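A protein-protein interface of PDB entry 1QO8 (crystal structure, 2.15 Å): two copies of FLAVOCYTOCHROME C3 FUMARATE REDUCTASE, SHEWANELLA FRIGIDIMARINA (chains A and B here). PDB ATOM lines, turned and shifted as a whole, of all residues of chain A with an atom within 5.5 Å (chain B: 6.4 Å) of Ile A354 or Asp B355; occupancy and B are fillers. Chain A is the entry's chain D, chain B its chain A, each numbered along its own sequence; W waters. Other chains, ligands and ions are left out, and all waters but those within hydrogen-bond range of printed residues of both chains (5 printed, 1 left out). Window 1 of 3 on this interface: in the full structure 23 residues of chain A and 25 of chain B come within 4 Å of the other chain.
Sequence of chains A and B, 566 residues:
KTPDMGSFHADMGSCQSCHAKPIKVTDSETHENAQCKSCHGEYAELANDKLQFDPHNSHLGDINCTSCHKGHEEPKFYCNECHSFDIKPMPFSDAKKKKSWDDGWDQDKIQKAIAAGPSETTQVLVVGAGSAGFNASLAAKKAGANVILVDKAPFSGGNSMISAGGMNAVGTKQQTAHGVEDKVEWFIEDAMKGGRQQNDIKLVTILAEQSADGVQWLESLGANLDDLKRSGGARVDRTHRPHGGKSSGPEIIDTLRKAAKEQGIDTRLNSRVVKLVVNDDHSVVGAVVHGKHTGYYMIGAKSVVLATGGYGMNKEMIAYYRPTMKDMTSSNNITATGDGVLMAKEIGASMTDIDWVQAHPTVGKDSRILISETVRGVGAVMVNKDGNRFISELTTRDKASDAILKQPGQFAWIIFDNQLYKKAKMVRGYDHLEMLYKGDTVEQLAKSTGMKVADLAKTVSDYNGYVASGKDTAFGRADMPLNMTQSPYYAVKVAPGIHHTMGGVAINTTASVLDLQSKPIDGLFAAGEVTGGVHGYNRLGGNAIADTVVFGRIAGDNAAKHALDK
The backbone carbonyl oxygen (O) of Trp B356 lies within hydrogen-bond range of the backbone NH (N) of Gly B503, at 3.3 Å. NH1 of Arg B322 lies within salt-bridge range of OD2 of Asp B355. OH of Tyr A311 sits at hydrogen-bond distance from O of Ile A354.
Among the printed residues, pairs that only touch across the chains: Tyr A321 with Tyr B320 (3.7 Å), Ser A350 with Trp B356 (3.7 Å), Met A351 with Asp B355 (3.7 Å) and Ile A354 with Asp B355 (3.9 Å).
Of chain B, only Asp B355 comes within 4 Å of Ile A354. Asp B355 touches just these residues of chain A: Met A351 and Ile A354. Printed residues of chain B within 4 Å of Ser A350: Trp B356. Printed residues of chain B within 4 Å of Tyr A321: Tyr B320. Of the printed residues of chain A, Tyr B320 touches Tyr A321 (3.7 Å). The nearest residue of chain B that does not touch Ile A354 is Ile B354 (4.2 Å). The nearest printed residue of chain A that does not touch Asp B355 is Ser A350 (5.5 Å). The nearest printed residue of chain A that does not touch Trp B356 is Met A351 (4.04 Å).
Printed residues of chain A that touch a printed residue of chain B: Tyr A321, Ser A350, Met A351 and Ile A354. Hydrophobic or aromatic side chains of chain A that line the printed part of chain B: Tyr A321, Met A351 and Ile A354. Along chain B the printed residues that touch a printed residue of chain A span positions 320 to 356. Among the printed residues, no Asp or Glu carboxylate lies within 4 Å of a Lys or Arg side-chain nitrogen of the other chain.
Ile A354 touches Asp B355, but with the chains exchanged Asp A355 does not touch Ile B354 (4.1 Å). Positions printed for both chains: 311, 321, 352, 353, 354, 355, 356, 503 and 504. Of the 4 pairs that touch across the chains among the printed residues, none has its exchanged pair printed and touching as well.
Water W5 lies within hydrogen-bond range of the side-chain hydroxyl of Tyr A321 and the side-chain hydroxyl of Tyr B320. Water W3 lies within hydrogen-bond range of the side-chain carboxylate of Asp B355 (2.6 Å), the backbone NH of Ile A354 (3.0 Å) and the backbone NH of Asp A353 (3.4 Å). Water W1 bridges the side-chain hydroxyl of Tyr A321 and the backbone carbonyl oxygen of Tyr B320. Water W2 lies within hydrogen-bond range of the backbone carbonyl oxygen of Met A351 (2.8 Å), the indole nitrogen of Trp B356 (3.1 Å) and the backbone NH of Asp A353 (3.5 Å). Water W4 lies within hydrogen-bond range of the side-chain carboxylate of Asp A355 (2.9 Å), the backbone NH of Ile B354 (3.0 Å) and the backbone NH of Asp B353 (3.3 Å).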
ATOM      1  N   TYR A 311       2.322 -18.639  -6.623  1.00  0.00           N
ATOM      2  CA  TYR A 311       2.483 -17.952  -7.927  1.00  0.00           C
ATOM      3  C   TYR A 311       3.030 -18.871  -8.948  1.00  0.00           C
ATOM      4  O   TYR A 311       3.467 -18.418 -10.045  1.00  0.00           O
ATOM      5  CB  TYR A 311       3.319 -16.666  -7.780  1.00  0.00           C
ATOM      6  CG  TYR A 311       4.750 -16.797  -7.301  1.00  0.00           C
ATOM      7  CD1 TYR A 311       5.738 -17.059  -8.201  1.00  0.00           C
ATOM      8  CD2 TYR A 311       5.132 -16.647  -5.966  1.00  0.00           C
ATOM      9  CE1 TYR A 311       7.081 -17.167  -7.816  1.00  0.00           C
ATOM     10  CE2 TYR A 311       6.422 -16.728  -5.530  1.00  0.00           C
ATOM     11  CZ  TYR A 311       7.394 -16.960  -6.494  1.00  0.00           C
ATOM     12  OH  TYR A 311       8.749 -17.061  -6.232  1.00  0.00           O
ATOM     13  N   TYR A 321      12.123 -14.697 -10.860  1.00  0.00           N
ATOM     14  CA  TYR A 321      12.682 -15.268  -9.651  1.00  0.00           C
ATOM     15  C   TYR A 321      13.552 -16.447  -9.935  1.00  0.00           C
ATOM     16  O   TYR A 321      14.503 -16.774  -9.189  1.00  0.00           O
ATOM     17  CB  TYR A 321      11.561 -15.649  -8.636  1.00  0.00           C
ATOM     18  CG  TYR A 321      10.772 -14.472  -8.122  1.00  0.00           C
ATOM     19  CD1 TYR A 321      11.464 -13.264  -7.800  1.00  0.00           C
ATOM     20  CD2 TYR A 321       9.433 -14.448  -7.905  1.00  0.00           C
ATOM     21  CE1 TYR A 321      10.769 -12.169  -7.261  1.00  0.00           C
ATOM     22  CE2 TYR A 321       8.724 -13.365  -7.372  1.00  0.00           C
ATOM     23  CZ  TYR A 321       9.444 -12.209  -7.074  1.00  0.00           C
ATOM     24  OH  TYR A 321       8.725 -11.119  -6.596  1.00  0.00           O
ATOM     25  N   VAL A 341       0.650 -11.516  -3.706  1.00  0.00           N
ATOM     26  CA  VAL A 341       2.031 -11.084  -3.653  1.00  0.00           C
ATOM     27  C   VAL A 341       2.123  -9.792  -4.479  1.00  0.00           C
ATOM     28  O   VAL A 341       2.617  -8.800  -3.957  1.00  0.00           O
ATOM     29  CB  VAL A 341       3.025 -12.150  -4.172  1.00  0.00           C
ATOM     30  CG1 VAL A 341       4.392 -11.636  -4.536  1.00  0.00           C
ATOM     31  CG2 VAL A 341       3.165 -13.283  -3.098  1.00  0.00           C
ATOM     32  N   SER A 350       6.681  -6.080   2.622  1.00  0.00           N
ATOM     33  CA  SER A 350       7.808  -6.939   2.486  1.00  0.00           C
ATOM     34  C   SER A 350       7.370  -8.385   2.249  1.00  0.00           C
ATOM     35  O   SER A 350       6.257  -8.791   2.539  1.00  0.00           O
ATOM     36  CB  SER A 350       8.733  -6.889   3.701  1.00  0.00           C
ATOM     37  OG  SER A 350       8.219  -7.210   4.969  1.00  0.00           O
ATOM     38  N   MET A 351       8.392  -9.132   1.804  1.00  0.00           N
ATOM     39  CA  MET A 351       8.191 -10.521   1.441  1.00  0.00           C
ATOM     40  C   MET A 351       9.138 -11.352   2.295  1.00  0.00           C
ATOM     41  O   MET A 351      10.112 -10.779   2.863  1.00  0.00           O
ATOM     42  CB  MET A 351       8.628 -10.707  -0.051  1.00  0.00           C
ATOM     43  CG  MET A 351       7.829  -9.748  -0.939  1.00  0.00           C
ATOM     44  SD  MET A 351       6.077 -10.200  -1.115  1.00  0.00           S
ATOM     45  CE  MET A 351       5.398  -8.563  -1.247  1.00  0.00           C
ATOM     46  N   THR A 352       8.908 -12.653   2.385  1.00  0.00           N
ATOM     47  CA  THR A 352       9.927 -13.489   3.009  1.00  0.00           C
ATOM     48  C   THR A 352      10.307 -14.552   1.986  1.00  0.00           C
ATOM     49  O   THR A 352       9.386 -15.155   1.373  1.00  0.00           O
ATOM     50  CB  THR A 352       9.289 -14.184   4.249  1.00  0.00           C
ATOM     51  OG1 THR A 352       8.925 -13.199   5.241  1.00  0.00           O
ATOM     52  CG2 THR A 352      10.193 -15.233   4.806  1.00  0.00           C
ATOM     53  N   ASP A 353      11.546 -14.962   1.902  1.00  0.00           N
ATOM     54  CA  ASP A 353      11.968 -15.984   0.945  1.00  0.00           C
ATOM     55  C   ASP A 353      11.365 -15.807  -0.431  1.00  0.00           C
ATOM     56  O   ASP A 353      11.099 -16.832  -1.109  1.00  0.00           O
ATOM     57  CB  ASP A 353      11.642 -17.378   1.582  1.00  0.00           C
ATOM     58  CG  ASP A 353      12.309 -17.534   2.934  1.00  0.00           C
ATOM     59  OD1 ASP A 353      13.355 -16.857   3.188  1.00  0.00           O
ATOM     60  OD2 ASP A 353      11.946 -18.316   3.822  1.00  0.00           O
ATOM     61  N   ILE A 354      11.194 -14.591  -1.012  1.00  0.00           N
ATOM     62  CA  ILE A 354      10.223 -14.439  -2.057  1.00  0.00           C
ATOM     63  C   ILE A 354      10.457 -15.322  -3.302  1.00  0.00           C
ATOM     64  O   ILE A 354       9.485 -15.820  -3.858  1.00  0.00           O
ATOM     65  CB  ILE A 354      10.102 -12.979  -2.510  1.00  0.00           C
ATOM     66  CG1 ILE A 354       9.007 -12.798  -3.584  1.00  0.00           C
ATOM     67  CG2 ILE A 354      11.467 -12.511  -3.027  1.00  0.00           C
ATOM     68  CD1 ILE A 354       7.627 -13.074  -3.036  1.00  0.00           C
ATOM     69  N   ASP A 355      11.670 -15.562  -3.751  1.00  0.00           N
ATOM     70  CA  ASP A 355      12.001 -16.294  -4.976  1.00  0.00           C
ATOM     71  C   ASP A 355      12.104 -17.812  -4.795  1.00  0.00           C
ATOM     72  O   ASP A 355      12.447 -18.509  -5.732  1.00  0.00           O
ATOM     73  CB  ASP A 355      13.290 -15.703  -5.567  1.00  0.00           C
ATOM     74  CG  ASP A 355      14.475 -15.706  -4.601  1.00  0.00           C
ATOM     75  OD1 ASP A 355      14.294 -15.690  -3.357  1.00  0.00           O
ATOM     76  OD2 ASP A 355      15.569 -15.752  -5.215  1.00  0.00           O
ATOM     77  N   TRP A 356      11.772 -18.376  -3.637  1.00  0.00           N
ATOM     78  CA  TRP A 356      11.939 -19.819  -3.430  1.00  0.00           C
ATOM     79  C   TRP A 356      10.773 -20.615  -4.013  1.00  0.00           C
ATOM     80  O   TRP A 356       9.637 -20.441  -3.572  1.00  0.00           O
ATOM     81  CB  TRP A 356      12.247 -20.189  -1.984  1.00  0.00           C
ATOM     82  CG  TRP A 356      13.695 -19.804  -1.739  1.00  0.00           C
ATOM     83  CD1 TRP A 356      14.141 -18.598  -1.230  1.00  0.00           C
ATOM     84  CD2 TRP A 356      14.846 -20.611  -2.018  1.00  0.00           C
ATOM     85  NE1 TRP A 356      15.498 -18.653  -1.189  1.00  0.00           N
ATOM     86  CE2 TRP A 356      15.987 -19.838  -1.664  1.00  0.00           C
ATOM     87  CE3 TRP A 356      15.031 -21.919  -2.500  1.00  0.00           C
ATOM     88  CZ2 TRP A 356      17.271 -20.314  -1.786  1.00  0.00           C
ATOM     89  CZ3 TRP A 356      16.321 -22.411  -2.651  1.00  0.00           C
ATOM     90  CH2 TRP A 356      17.447 -21.614  -2.262  1.00  0.00           C
ATOM     91  N   GLY A 503       7.957 -18.877  -1.101  1.00  0.00           N
ATOM     92  CA  GLY A 503       8.087 -17.476  -0.711  1.00  0.00           C
ATOM     93  C   GLY A 503       6.670 -16.848  -0.821  1.00  0.00           C
ATOM     94  O   GLY A 503       5.801 -17.389  -1.490  1.00  0.00           O
ATOM     95  N   GLY A 504       6.587 -15.633  -0.340  1.00  0.00           N
ATOM     96  CA  GLY A 504       5.391 -14.834  -0.409  1.00  0.00           C
ATOM     97  C   GLY A 504       5.537 -13.660   0.563  1.00  0.00           C
ATOM     98  O   GLY A 504       6.628 -13.330   1.045  1.00  0.00           O
ATOM     99  N   VAL A 505       4.408 -13.081   0.884  1.00  0.00           N
ATOM    100  CA  VAL A 505       4.226 -11.954   1.769  1.00  0.00           C
ATOM    101  C   VAL A 505       4.841 -12.290   3.110  1.00  0.00           C
ATOM    102  O   VAL A 505       4.717 -13.430   3.568  1.00  0.00           O
ATOM    103  CB  VAL A 505       2.703 -11.851   1.631  1.00  0.00           C
ATOM    104  CG1 VAL A 505       1.843 -11.764   2.854  1.00  0.00           C
ATOM    105  CG2 VAL A 505       2.423 -10.914   0.467  1.00  0.00           C
ATOM    106  N   TYR B 311      23.069  -3.403  -6.431  1.00  0.00           N
ATOM    107  CA  TYR B 311      22.180  -3.247  -7.573  1.00  0.00           C
ATOM    108  C   TYR B 311      21.372  -1.955  -7.389  1.00  0.00           C
ATOM    109  O   TYR B 311      20.460  -1.634  -8.187  1.00  0.00           O
ATOM    110  CB  TYR B 311      21.252  -4.419  -7.840  1.00  0.00           C
ATOM    111  CG  TYR B 311      20.224  -4.892  -6.833  1.00  0.00           C
ATOM    112  CD1 TYR B 311      18.964  -4.248  -6.820  1.00  0.00           C
ATOM    113  CD2 TYR B 311      20.433  -5.879  -5.901  1.00  0.00           C
ATOM    114  CE1 TYR B 311      17.992  -4.584  -5.892  1.00  0.00           C
ATOM    115  CE2 TYR B 311      19.433  -6.276  -5.006  1.00  0.00           C
ATOM    116  CZ  TYR B 311      18.209  -5.617  -5.021  1.00  0.00           C
ATOM    117  OH  TYR B 311      17.183  -5.966  -4.180  1.00  0.00           O
ATOM    118  N   TYR B 320      11.317  -3.868  -9.471  1.00  0.00           N
ATOM    119  CA  TYR B 320      10.780  -5.194  -9.275  1.00  0.00           C
ATOM    120  C   TYR B 320      10.765  -5.696  -7.838  1.00  0.00           C
ATOM    121  O   TYR B 320       9.833  -6.384  -7.379  1.00  0.00           O
ATOM    122  CB  TYR B 320      11.517  -6.249 -10.131  1.00  0.00           C
ATOM    123  CG  TYR B 320      10.471  -7.356 -10.363  1.00  0.00           C
ATOM    124  CD1 TYR B 320       9.428  -7.187 -11.275  1.00  0.00           C
ATOM    125  CD2 TYR B 320      10.550  -8.481  -9.585  1.00  0.00           C
ATOM    126  CE1 TYR B 320       8.465  -8.208 -11.430  1.00  0.00           C
ATOM    127  CE2 TYR B 320       9.611  -9.496  -9.748  1.00  0.00           C
ATOM    128  CZ  TYR B 320       8.598  -9.362 -10.676  1.00  0.00           C
ATOM    129  OH  TYR B 320       7.692 -10.378 -10.765  1.00  0.00           O
ATOM    130  N   TYR B 321      11.807  -5.438  -7.092  1.00  0.00           N
ATOM    131  CA  TYR B 321      11.965  -5.929  -5.732  1.00  0.00           C
ATOM    132  C   TYR B 321      11.313  -4.948  -4.764  1.00  0.00           C
ATOM    133  O   TYR B 321      10.831  -5.337  -3.703  1.00  0.00           O
ATOM    134  CB  TYR B 321      13.449  -6.105  -5.407  1.00  0.00           C
ATOM    135  CG  TYR B 321      14.207  -7.177  -6.162  1.00  0.00           C
ATOM    136  CD1 TYR B 321      13.593  -8.425  -6.312  1.00  0.00           C
ATOM    137  CD2 TYR B 321      15.458  -6.998  -6.747  1.00  0.00           C
ATOM    138  CE1 TYR B 321      14.244  -9.464  -6.961  1.00  0.00           C
ATOM    139  CE2 TYR B 321      16.095  -8.044  -7.413  1.00  0.00           C
ATOM    140  CZ  TYR B 321      15.479  -9.281  -7.530  1.00  0.00           C
ATOM    141  OH  TYR B 321      16.069 -10.335  -8.157  1.00  0.00           O
ATOM    142  N   ARG B 322      11.373  -3.631  -5.042  1.00  0.00           N
ATOM    143  CA  ARG B 322      10.982  -2.612  -4.078  1.00  0.00           C
ATOM    144  C   ARG B 322      10.337  -1.451  -4.818  1.00  0.00           C
ATOM    145  O   ARG B 322      10.883  -0.339  -4.864  1.00  0.00           O
ATOM    146  CB  ARG B 322      12.209  -2.045  -3.293  1.00  0.00           C
ATOM    147  CG  ARG B 322      12.752  -2.971  -2.214  1.00  0.00           C
ATOM    148  CD  ARG B 322      11.726  -2.947  -1.034  1.00  0.00           C
ATOM    149  NE  ARG B 322      12.216  -3.813   0.052  1.00  0.00           N
ATOM    150  CZ  ARG B 322      11.913  -5.131   0.074  1.00  0.00           C
ATOM    151  NH1 ARG B 322      11.151  -5.608  -0.893  1.00  0.00           N
ATOM    152  NH2 ARG B 322      12.385  -5.888   1.069  1.00  0.00           N
ATOM    153  N   THR B 352      20.087 -14.703  -1.558  1.00  0.00           N
ATOM    154  CA  THR B 352      19.760 -14.598  -0.105  1.00  0.00           C
ATOM    155  C   THR B 352      19.133 -13.230   0.146  1.00  0.00           C
ATOM    156  O   THR B 352      19.763 -12.178  -0.220  1.00  0.00           O
ATOM    157  CB  THR B 352      21.011 -14.772   0.777  1.00  0.00           C
ATOM    158  OG1 THR B 352      21.589 -16.073   0.654  1.00  0.00           O
ATOM    159  CG2 THR B 352      20.748 -14.579   2.282  1.00  0.00           C
ATOM    160  N   ASP B 353      17.978 -13.170   0.802  1.00  0.00           N
ATOM    161  CA  ASP B 353      17.331 -11.886   1.067  1.00  0.00           C
ATOM    162  C   ASP B 353      17.369 -10.947  -0.124  1.00  0.00           C
ATOM    163  O   ASP B 353      17.614  -9.705   0.031  1.00  0.00           O
ATOM    164  CB  ASP B 353      17.953 -11.144   2.298  1.00  0.00           C
ATOM    165  CG  ASP B 353      18.086 -11.986   3.544  1.00  0.00           C
ATOM    166  OD1 ASP B 353      17.138 -12.792   3.813  1.00  0.00           O
ATOM    167  OD2 ASP B 353      19.071 -11.921   4.319  1.00  0.00           O
ATOM    168  N   ILE B 354      16.987 -11.421  -1.329  1.00  0.00           N
ATOM    169  CA  ILE B 354      17.431 -10.762  -2.566  1.00  0.00           C
ATOM    170  C   ILE B 354      16.863  -9.356  -2.683  1.00  0.00           C
ATOM    171  O   ILE B 354      17.435  -8.360  -3.180  1.00  0.00           O
ATOM    172  CB  ILE B 354      17.057 -11.605  -3.785  1.00  0.00           C
ATOM    173  CG1 ILE B 354      17.534 -11.032  -5.118  1.00  0.00           C
ATOM    174  CG2 ILE B 354      15.537 -11.811  -3.830  1.00  0.00           C
ATOM    175  CD1 ILE B 354      19.065 -10.972  -5.266  1.00  0.00           C
ATOM    176  N   ASP B 355      15.665  -9.188  -2.107  1.00  0.00           N
ATOM    177  CA  ASP B 355      14.893  -7.962  -2.350  1.00  0.00           C
ATOM    178  C   ASP B 355      15.131  -6.900  -1.264  1.00  0.00           C
ATOM    179  O   ASP B 355      14.502  -5.838  -1.381  1.00  0.00           O
ATOM    180  CB  ASP B 355      13.421  -8.275  -2.546  1.00  0.00           C
ATOM    181  CG  ASP B 355      12.662  -9.028  -1.482  1.00  0.00           C
ATOM    182  OD1 ASP B 355      13.283  -9.834  -0.768  1.00  0.00           O
ATOM    183  OD2 ASP B 355      11.445  -8.788  -1.364  1.00  0.00           O
ATOM    184  N   TRP B 356      16.086  -7.026  -0.385  1.00  0.00           N
ATOM    185  CA  TRP B 356      16.225  -6.152   0.796  1.00  0.00           C
ATOM    186  C   TRP B 356      17.149  -4.964   0.446  1.00  0.00           C
ATOM    187  O   TRP B 356      18.298  -5.237   0.057  1.00  0.00           O
ATOM    188  CB  TRP B 356      16.652  -6.892   2.090  1.00  0.00           C
ATOM    189  CG  TRP B 356      15.405  -7.546   2.637  1.00  0.00           C
ATOM    190  CD1 TRP B 356      14.963  -8.816   2.388  1.00  0.00           C
ATOM    191  CD2 TRP B 356      14.419  -6.944   3.471  1.00  0.00           C
ATOM    192  NE1 TRP B 356      13.760  -9.061   3.014  1.00  0.00           N
ATOM    193  CE2 TRP B 356      13.403  -7.913   3.670  1.00  0.00           C
ATOM    194  CE3 TRP B 356      14.285  -5.669   4.020  1.00  0.00           C
ATOM    195  CZ2 TRP B 356      12.257  -7.632   4.424  1.00  0.00           C
ATOM    196  CZ3 TRP B 356      13.132  -5.390   4.745  1.00  0.00           C
ATOM    197  CH2 TRP B 356      12.171  -6.384   4.981  1.00  0.00           C
ATOM    198  N   VAL B 357      16.547  -3.791   0.303  1.00  0.00           N
ATOM    199  CA  VAL B 357      17.202  -2.565  -0.137  1.00  0.00           C
ATOM    200  C   VAL B 357      17.112  -1.453   0.941  1.00  0.00           C
ATOM    201  O   VAL B 357      16.113  -1.149   1.621  1.00  0.00           O
ATOM    202  CB  VAL B 357      16.610  -2.071  -1.462  1.00  0.00           C
ATOM    203  CG1 VAL B 357      17.267  -0.786  -1.992  1.00  0.00           C
ATOM    204  CG2 VAL B 357      16.676  -3.214  -2.505  1.00  0.00           C
ATOM    205  N   GLY B 503      20.604  -7.652  -0.116  1.00  0.00           N
ATOM    206  CA  GLY B 503      20.385  -8.959  -0.674  1.00  0.00           C
ATOM    207  C   GLY B 503      21.367  -9.205  -1.836  1.00  0.00           C
ATOM    208  O   GLY B 503      21.986  -8.234  -2.348  1.00  0.00           O
ATOM    209  N   GLY B 504      21.521 -10.459  -2.202  1.00  0.00           N
ATOM    210  CA  GLY B 504      22.369 -10.730  -3.380  1.00  0.00           C
ATOM    211  C   GLY B 504      22.457 -12.265  -3.545  1.00  0.00           C
ATOM    212  O   GLY B 504      21.615 -12.996  -3.056  1.00  0.00           O
HETATM  213  O   HOH W   1      10.008  -8.907  -5.878  1.00  0.00           O
HETATM  214  O   HOH W   2      12.694 -11.928   3.146  1.00  0.00           O
HETATM  215  O   HOH W   3      12.393 -12.075   0.221  1.00  0.00           O
HETATM  216  O   HOH W   4      16.191 -14.295  -1.724  1.00  0.00           O
HETATM  217  O   HOH W   5       6.817 -10.126  -8.016  1.00  0.00           O
